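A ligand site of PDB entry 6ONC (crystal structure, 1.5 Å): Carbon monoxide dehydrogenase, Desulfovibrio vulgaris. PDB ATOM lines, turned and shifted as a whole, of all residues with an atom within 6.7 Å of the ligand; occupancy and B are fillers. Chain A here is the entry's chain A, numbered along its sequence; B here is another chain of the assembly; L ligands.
The side-chain sulfur of Cys 59 binds an iron atom (FE1) of the ligand, at 2.3 Å. The side-chain sulfur of Cys 82 is bound to an iron atom (FE3) of the ligand, at 2.3 Å. N of Cys 62 lies close to S3 of the ligand (3.7 Å). A sulfur (S1) of the ligand sits close to the backbone NH of Val 81 (3.8 Å). The side-chain sulfur (SG) of Cys 67 binds an iron atom (FE2) of the ligand (2.3 Å). The guanidinium group of Arg 92 sits close to a sulfur (S2) of the ligand (3.6 Å). The backbone NH (N) of Cys 82 lies close to a sulfur (S1) of the ligand (3.3 Å). The side-chain sulfur (SG) of Cys 62 is bound to an iron atom (FE4) of the ligand. A sulfur (S3) of the ligand sits close to the backbone NH (N) of Asn 61, 3.7 Å away.
The side-chain hydroxyl of Tyr 561 of chain B lies close to the side-chain sulfur of Met 211 (3.7 Å). The backbone NH (N) of Cys 59 is in hydrogen-bond range of the backbone carbonyl oxygen (O) of Cys 67 (2.9 Å). The side-chain sulfur (SG) of Cys 59 sits close to the guanidinium group (NH2) of Arg 92 (3.5 Å). SG of Cys 62 sits close to N of Met 64, 3.4 Å away. N of Val 81 sits close to SG of Cys 67 (3.4 Å). The side-chain sulfur of Cys 82 sits close to the backbone NH of Ala 84. O of Cys 67 lies close to OG1 of Thr 58. N of Asn 61 lies close to SG of Cys 59 (3.6 Å).
Met 64 touches the ligand. CA of Gly 65 touches S3 of the ligand (3.8 Å). CA of Gly 80 touches S4 of the ligand (3.9 Å). Ile 89 touches the ligand (CD1 to S4, 3.9 Å). Met 211 touches the ligand (CG to S2, 3.7 Å). Hydrophobic or aromatic side chains within 4 Å of the ligand: Met 64, Val 81, Ile 89 and Met 211. Along chain A the residues within 4 Å of the ligand span positions 59 to 211.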
ATOM      1  N   THR A  58      14.526  -1.858   0.657  1.00  0.00           N
ATOM      2  CA  THR A  58      13.416  -1.473   1.523  1.00  0.00           C
ATOM      3  C   THR A  58      13.043  -0.033   1.193  1.00  0.00           C
ATOM      4  O   THR A  58      13.906   0.796   0.921  1.00  0.00           O
ATOM      5  CB  THR A  58      13.787  -1.600   3.011  1.00  0.00           C
ATOM      6  OG1 THR A  58      12.751  -1.027   3.817  1.00  0.00           O
ATOM      7  CG2 THR A  58      15.114  -0.908   3.300  1.00  0.00           C
ATOM      8  N   CYS A  59      11.740   0.254   1.201  1.00  0.00           N
ATOM      9  CA  CYS A  59      11.284   1.581   0.805  1.00  0.00           C
ATOM     10  C   CYS A  59      10.210   2.048   1.768  1.00  0.00           C
ATOM     11  O   CYS A  59       9.305   1.291   2.125  1.00  0.00           O
ATOM     12  CB  CYS A  59      10.731   1.567  -0.632  1.00  0.00           C
ATOM     13  SG  CYS A  59      10.263   3.189  -1.277  1.00  0.00           S
ATOM     14  N   ARG A  60      10.318   3.312   2.186  1.00  0.00           N
ATOM     15  CA  ARG A  60       9.376   3.940   3.099  1.00  0.00           C
ATOM     16  C   ARG A  60       8.878   5.265   2.543  1.00  0.00           C
ATOM     17  O   ARG A  60       8.536   6.176   3.301  1.00  0.00           O
ATOM     18  CB  ARG A  60      10.003   4.134   4.481  1.00  0.00           C
ATOM     19  CG  ARG A  60      10.563   2.854   5.087  1.00  0.00           C
ATOM     20  CD  ARG A  60      11.319   3.089   6.392  1.00  0.00           C
ATOM     21  NE  ARG A  60      12.640   3.668   6.196  1.00  0.00           N
ATOM     22  CZ  ARG A  60      13.074   4.774   6.795  1.00  0.00           C
ATOM     23  NH1 ARG A  60      12.276   5.418   7.645  1.00  0.00           N
ATOM     24  NH2 ARG A  60      14.293   5.226   6.568  1.00  0.00           N
ATOM     25  N   ASN A  61       8.833   5.399   1.221  1.00  0.00           N
ATOM     26  CA  ASN A  61       8.533   6.682   0.581  1.00  0.00           C
ATOM     27  C   ASN A  61       7.029   6.985   0.474  1.00  0.00           C
ATOM     28  O   ASN A  61       6.677   8.065  -0.015  1.00  0.00           O
ATOM     29  CB  ASN A  61       9.200   6.799  -0.801  1.00  0.00           C
ATOM     30  CG  ASN A  61      10.718   6.907  -0.726  1.00  0.00           C
ATOM     31  OD1 ASN A  61      11.382   7.219  -1.721  1.00  0.00           O
ATOM     32  ND2 ASN A  61      11.273   6.616   0.431  1.00  0.00           N
ATOM     33  N   CYS A  62       6.163   6.079   0.891  1.00  0.00           N
ATOM     34  CA  CYS A  62       4.723   6.356   0.951  1.00  0.00           C
ATOM     35  C   CYS A  62       4.091   5.336   1.886  1.00  0.00           C
ATOM     36  O   CYS A  62       4.724   4.332   2.247  1.00  0.00           O
ATOM     37  CB  CYS A  62       4.075   6.323  -0.434  1.00  0.00           C
ATOM     38  SG  CYS A  62       3.663   4.671  -1.073  1.00  0.00           S
ATOM     39  N   ILE A  63       2.849   5.583   2.293  1.00  0.00           N
ATOM     40  CA  ILE A  63       2.160   4.680   3.213  1.00  0.00           C
ATOM     41  C   ILE A  63       1.228   3.692   2.496  1.00  0.00           C
ATOM     42  O   ILE A  63       0.377   3.075   3.145  1.00  0.00           O
ATOM     43  CB  ILE A  63       1.491   5.384   4.412  1.00  0.00           C
ATOM     44  CG1 ILE A  63       0.283   6.213   3.974  1.00  0.00           C
ATOM     45  CG2 ILE A  63       2.519   6.240   5.174  1.00  0.00           C
ATOM     46  CD1 ILE A  63      -0.837   6.245   5.010  1.00  0.00           C
ATOM     47  N   MET A  64       1.373   3.524   1.181  1.00  0.00           N
ATOM     48  CA  MET A  64       0.984   2.243   0.616  1.00  0.00           C
ATOM     49  C   MET A  64       1.933   1.155   1.107  1.00  0.00           C
ATOM     50  O   MET A  64       1.533  -0.003   1.262  1.00  0.00           O
ATOM     51  CB  MET A  64       0.978   2.269  -0.910  1.00  0.00           C
ATOM     52  CG  MET A  64      -0.045   3.216  -1.517  1.00  0.00           C
ATOM     53  SD  MET A  64      -0.516   2.717  -3.209  1.00  0.00           S
ATOM     54  CE  MET A  64       1.067   2.792  -4.060  1.00  0.00           C
ATOM     55  N   GLY A  65       3.190   1.528   1.353  1.00  0.00           N
ATOM     56  CA  GLY A  65       4.160   0.679   1.989  1.00  0.00           C
ATOM     57  C   GLY A  65       4.087   0.790   3.498  1.00  0.00           C
ATOM     58  O   GLY A  65       3.036   1.132   4.054  1.00  0.00           O
ATOM     59  N   PRO A  66       5.201   0.534   4.205  1.00  0.00           N
ATOM     60  CA  PRO A  66       6.547   0.279   3.678  1.00  0.00           C
ATOM     61  C   PRO A  66       6.686  -1.065   2.989  1.00  0.00           C
ATOM     62  O   PRO A  66       5.935  -2.009   3.254  1.00  0.00           O
ATOM     63  CB  PRO A  66       7.426   0.311   4.945  1.00  0.00           C
ATOM     64  CG  PRO A  66       6.512  -0.111   6.027  1.00  0.00           C
ATOM     65  CD  PRO A  66       5.174   0.496   5.674  1.00  0.00           C
ATOM     66  N   CYS A  67       7.668  -1.125   2.090  1.00  0.00           N
ATOM     67  CA  CYS A  67       7.865  -2.277   1.231  1.00  0.00           C
ATOM     68  C   CYS A  67       9.249  -2.857   1.448  1.00  0.00           C
ATOM     69  O   CYS A  67      10.199  -2.132   1.800  1.00  0.00           O
ATOM     70  CB  CYS A  67       7.696  -1.891  -0.246  1.00  0.00           C
ATOM     71  SG  CYS A  67       6.032  -1.230  -0.602  1.00  0.00           S
ATOM     72  N   ARG A  68       9.365  -4.170   1.246  1.00  0.00           N
ATOM     73  CA  ARG A  68      10.646  -4.853   1.179  1.00  0.00           C
ATOM     74  C   ARG A  68      10.685  -5.700  -0.078  1.00  0.00           C
ATOM     75  O   ARG A  68       9.669  -6.287  -0.466  1.00  0.00           O
ATOM     76  CB  ARG A  68      10.847  -5.767   2.391  1.00  0.00           C
ATOM     77  CG  ARG A  68      11.192  -5.000   3.662  1.00  0.00           C
ATOM     78  CD  ARG A  68      10.940  -5.834   4.882  1.00  0.00           C
ATOM     79  NE  ARG A  68       9.517  -6.113   5.024  1.00  0.00           N
ATOM     80  CZ  ARG A  68       9.023  -7.211   5.581  1.00  0.00           C
ATOM     81  NH1 ARG A  68       9.832  -8.134   6.085  1.00  0.00           N
ATOM     82  NH2 ARG A  68       7.713  -7.390   5.628  1.00  0.00           N
ATOM     83  N   ILE A  69      11.837  -5.764  -0.719  1.00  0.00           N
ATOM     84  CA  ILE A  69      12.016  -6.581  -1.915  1.00  0.00           C
ATOM     85  C   ILE A  69      12.794  -7.819  -1.509  1.00  0.00           C
ATOM     86  O   ILE A  69      13.921  -7.713  -1.018  1.00  0.00           O
ATOM     87  CB  ILE A  69      12.715  -5.816  -3.050  1.00  0.00           C
ATOM     88  CG1 ILE A  69      11.967  -4.508  -3.360  1.00  0.00           C
ATOM     89  CG2 ILE A  69      12.796  -6.672  -4.305  1.00  0.00           C
ATOM     90  CD1 ILE A  69      10.525  -4.708  -3.792  1.00  0.00           C
ATOM     91  N   LEU A  79       8.173  -6.870  -6.038  1.00  0.00           N
ATOM     92  CA  LEU A  79       7.913  -5.457  -6.304  1.00  0.00           C
ATOM     93  C   LEU A  79       7.243  -4.810  -5.104  1.00  0.00           C
ATOM     94  O   LEU A  79       6.574  -5.474  -4.312  1.00  0.00           O
ATOM     95  CB  LEU A  79       6.969  -5.304  -7.510  1.00  0.00           C
ATOM     96  CG  LEU A  79       7.390  -5.999  -8.792  1.00  0.00           C
ATOM     97  CD1 LEU A  79       6.215  -6.004  -9.776  1.00  0.00           C
ATOM     98  CD2 LEU A  79       8.606  -5.327  -9.413  1.00  0.00           C
ATOM     99  N   GLY A  80       7.411  -3.491  -4.989  1.00  0.00           N
ATOM    100  CA  GLY A  80       6.682  -2.727  -4.002  1.00  0.00           C
ATOM    101  C   GLY A  80       5.217  -2.586  -4.404  1.00  0.00           C
ATOM    102  O   GLY A  80       4.791  -2.998  -5.483  1.00  0.00           O
ATOM    103  N   VAL A  81       4.430  -1.983  -3.506  1.00  0.00           N
ATOM    104  CA  VAL A  81       2.992  -1.879  -3.739  1.00  0.00           C
ATOM    105  C   VAL A  81       2.695  -1.064  -4.992  1.00  0.00           C
ATOM    106  O   VAL A  81       1.751  -1.360  -5.740  1.00  0.00           O
ATOM    107  CB  VAL A  81       2.277  -1.330  -2.485  1.00  0.00           C
ATOM    108  CG1 VAL A  81       0.773  -1.112  -2.756  1.00  0.00           C
ATOM    109  CG2 VAL A  81       2.458  -2.304  -1.335  1.00  0.00           C
ATOM    110  N   CYS A  82       3.522  -0.048  -5.281  1.00  0.00           N
ATOM    111  CA  CYS A  82       3.364   0.757  -6.482  1.00  0.00           C
ATOM    112  C   CYS A  82       3.879   0.080  -7.741  1.00  0.00           C
ATOM    113  O   CYS A  82       3.693   0.636  -8.832  1.00  0.00           O
ATOM    114  CB  CYS A  82       4.060   2.108  -6.332  1.00  0.00           C
ATOM    115  SG  CYS A  82       5.863   1.953  -6.133  1.00  0.00           S
ATOM    116  N   GLY A  83       4.519  -1.084  -7.631  1.00  0.00           N
ATOM    117  CA  GLY A  83       5.131  -1.757  -8.753  1.00  0.00           C
ATOM    118  C   GLY A  83       6.631  -1.557  -8.896  1.00  0.00           C
ATOM    119  O   GLY A  83       7.226  -2.137  -9.799  1.00  0.00           O
ATOM    120  N   ALA A  84       7.254  -0.752  -8.051  1.00  0.00           N
ATOM    121  CA  ALA A  84       8.674  -0.470  -8.227  1.00  0.00           C
ATOM    122  C   ALA A  84       9.509  -1.707  -7.902  1.00  0.00           C
ATOM    123  O   ALA A  84       9.221  -2.438  -6.954  1.00  0.00           O
ATOM    124  CB  ALA A  84       9.082   0.708  -7.347  1.00  0.00           C
ATOM    125  N   ILE A  89      14.034   1.046  -6.363  1.00  0.00           N
ATOM    126  CA  ILE A  89      14.048   1.305  -4.926  1.00  0.00           C
ATOM    127  C   ILE A  89      15.467   1.592  -4.444  1.00  0.00           C
ATOM    128  O   ILE A  89      15.698   2.550  -3.707  1.00  0.00           O
ATOM    129  CB  ILE A  89      13.388   0.143  -4.151  1.00  0.00           C
ATOM    130  CG1 ILE A  89      11.882   0.204  -4.353  1.00  0.00           C
ATOM    131  CG2 ILE A  89      13.775   0.196  -2.656  1.00  0.00           C
ATOM    132  CD1 ILE A  89      11.174  -1.104  -4.056  1.00  0.00           C
ATOM    133  N   ARG A  92      16.668   5.004  -5.897  1.00  0.00           N
ATOM    134  CA  ARG A  92      16.025   6.104  -5.192  1.00  0.00           C
ATOM    135  C   ARG A  92      16.624   6.289  -3.803  1.00  0.00           C
ATOM    136  O   ARG A  92      16.886   7.420  -3.385  1.00  0.00           O
ATOM    137  CB  ARG A  92      14.521   5.882  -5.086  1.00  0.00           C
ATOM    138  CG  ARG A  92      13.781   6.049  -6.400  1.00  0.00           C
ATOM    139  CD  ARG A  92      12.274   6.090  -6.185  1.00  0.00           C
ATOM    140  NE  ARG A  92      11.776   4.954  -5.416  1.00  0.00           N
ATOM    141  CZ  ARG A  92      10.530   4.504  -5.518  1.00  0.00           C
ATOM    142  NH1 ARG A  92       9.702   5.080  -6.391  1.00  0.00           N
ATOM    143  NH2 ARG A  92      10.108   3.473  -4.792  1.00  0.00           N
ATOM    144  N   THR A 209      12.402  11.072  -6.500  1.00  0.00           N
ATOM    145  CA  THR A 209      12.323   9.900  -5.646  1.00  0.00           C
ATOM    146  C   THR A 209      10.968   9.729  -4.955  1.00  0.00           C
ATOM    147  O   THR A 209      10.785   8.729  -4.252  1.00  0.00           O
ATOM    148  CB  THR A 209      13.478   9.891  -4.643  1.00  0.00           C
ATOM    149  OG1 THR A 209      13.521  11.169  -3.980  1.00  0.00           O
ATOM    150  CG2 THR A 209      14.814   9.657  -5.371  1.00  0.00           C
ATOM    151  N   HIS A 210      10.038  10.672  -5.122  1.00  0.00           N
ATOM    152  CA  HIS A 210       8.643  10.475  -4.726  1.00  0.00           C
ATOM    153  C   HIS A 210       8.065   9.305  -5.522  1.00  0.00           C
ATOM    154  O   HIS A 210       8.481   9.019  -6.643  1.00  0.00           O
ATOM    155  CB  HIS A 210       7.838  11.752  -5.045  1.00  0.00           C
ATOM    156  CG  HIS A 210       6.461  11.801  -4.451  1.00  0.00           C
ATOM    157  ND1 HIS A 210       5.392  11.103  -4.965  1.00  0.00           N
ATOM    158  CD2 HIS A 210       5.964  12.524  -3.411  1.00  0.00           C
ATOM    159  CE1 HIS A 210       4.304  11.355  -4.245  1.00  0.00           C
ATOM    160  NE2 HIS A 210       4.637  12.222  -3.296  1.00  0.00           N
ATOM    161  N   MET A 211       7.088   8.607  -4.922  1.00  0.00           N
ATOM    162  CA  MET A 211       6.411   7.535  -5.644  1.00  0.00           C
ATOM    163  C   MET A 211       5.952   8.014  -7.020  1.00  0.00           C
ATOM    164  O   MET A 211       5.381   9.097  -7.153  1.00  0.00           O
ATOM    165  CB  MET A 211       5.174   7.060  -4.865  1.00  0.00           C
ATOM    166  CG  MET A 211       4.524   5.768  -5.409  1.00  0.00           C
ATOM    167  SD  MET A 211       3.626   5.857  -7.001  1.00  0.00           S
ATOM    168  CE  MET A 211       1.914   5.697  -6.501  1.00  0.00           C
ATOM    169  N   GLY A 212       6.196   7.185  -8.025  1.00  0.00           N
ATOM    170  CA  GLY A 212       5.628   7.440  -9.341  1.00  0.00           C
ATOM    171  C   GLY A 212       6.206   8.625 -10.072  1.00  0.00           C
ATOM    172  O   GLY A 212       5.518   9.224 -10.897  1.00  0.00           O
ATOM    173  N   GLN B  46       2.850  -7.390   0.555  1.00  0.00           N
ATOM    174  CA  GLN B  46       3.640  -6.563   1.463  1.00  0.00           C
ATOM    175  C   GLN B  46       3.048  -6.478   2.867  1.00  0.00           C
ATOM    176  O   GLN B  46       3.519  -5.664   3.678  1.00  0.00           O
ATOM    177  CB  GLN B  46       3.849  -5.172   0.872  1.00  0.00           C
ATOM    178  CG  GLN B  46       4.701  -5.160  -0.407  1.00  0.00           C
ATOM    179  CD  GLN B  46       6.183  -5.463  -0.141  1.00  0.00           C
ATOM    180  OE1 GLN B  46       6.653  -5.399   0.994  1.00  0.00           O
ATOM    181  NE2 GLN B  46       6.915  -5.782  -1.203  1.00  0.00           N
ATOM    182  N   PRO B 351       4.636   2.458 -11.634  1.00  0.00           N
ATOM    183  CA  PRO B 351       5.365   1.772 -12.709  1.00  0.00           C
ATOM    184  C   PRO B 351       4.740   0.462 -13.128  1.00  0.00           C
ATOM    185  O   PRO B 351       5.073  -0.040 -14.195  1.00  0.00           O
ATOM    186  CB  PRO B 351       6.776   1.566 -12.115  1.00  0.00           C
ATOM    187  CG  PRO B 351       6.566   1.644 -10.633  1.00  0.00           C
ATOM    188  CD  PRO B 351       5.481   2.685 -10.448  1.00  0.00           C
ATOM    189  N   TYR B 561      -2.035   8.493   0.820  1.00  0.00           N
ATOM    190  CA  TYR B 561      -0.880   7.605   0.712  1.00  0.00           C
ATOM    191  C   TYR B 561       0.446   8.354   0.546  1.00  0.00           C
ATOM    192  O   TYR B 561       1.460   7.845   1.009  1.00  0.00           O
ATOM    193  CB  TYR B 561      -1.047   6.573  -0.450  1.00  0.00           C
ATOM    194  CG  TYR B 561      -0.332   7.035  -1.704  1.00  0.00           C
ATOM    195  CD1 TYR B 561       1.013   6.753  -1.884  1.00  0.00           C
ATOM    196  CD2 TYR B 561      -0.982   7.821  -2.668  1.00  0.00           C
ATOM    197  CE1 TYR B 561       1.707   7.222  -2.967  1.00  0.00           C
ATOM    198  CE2 TYR B 561      -0.277   8.293  -3.787  1.00  0.00           C
ATOM    199  CZ  TYR B 561       1.073   7.998  -3.910  1.00  0.00           C
ATOM    200  OH  TYR B 561       1.840   8.448  -4.972  1.00  0.00           O
HETATM  201 FE1  LIG L   1       8.120   2.793  -1.853  1.00  0.00          FE
HETATM  202 FE2  LIG L   1       6.299   0.842  -1.481  1.00  0.00          FE
HETATM  203 FE3  LIG L   1       6.370   2.216  -3.899  1.00  0.00          FE
HETATM  204 FE4  LIG L   1       5.508   3.469  -1.565  1.00  0.00          FE
HETATM  205  S1  LIG L   1       4.508   1.668  -2.609  1.00  0.00           S
HETATM  206  S2  LIG L   1       7.003   4.300  -3.116  1.00  0.00           S
HETATM  207  S3  LIG L   1       6.818   2.503   0.010  1.00  0.00           S
HETATM  208  S4  LIG L   1       7.985   0.845  -3.050  1.00  0.00           S
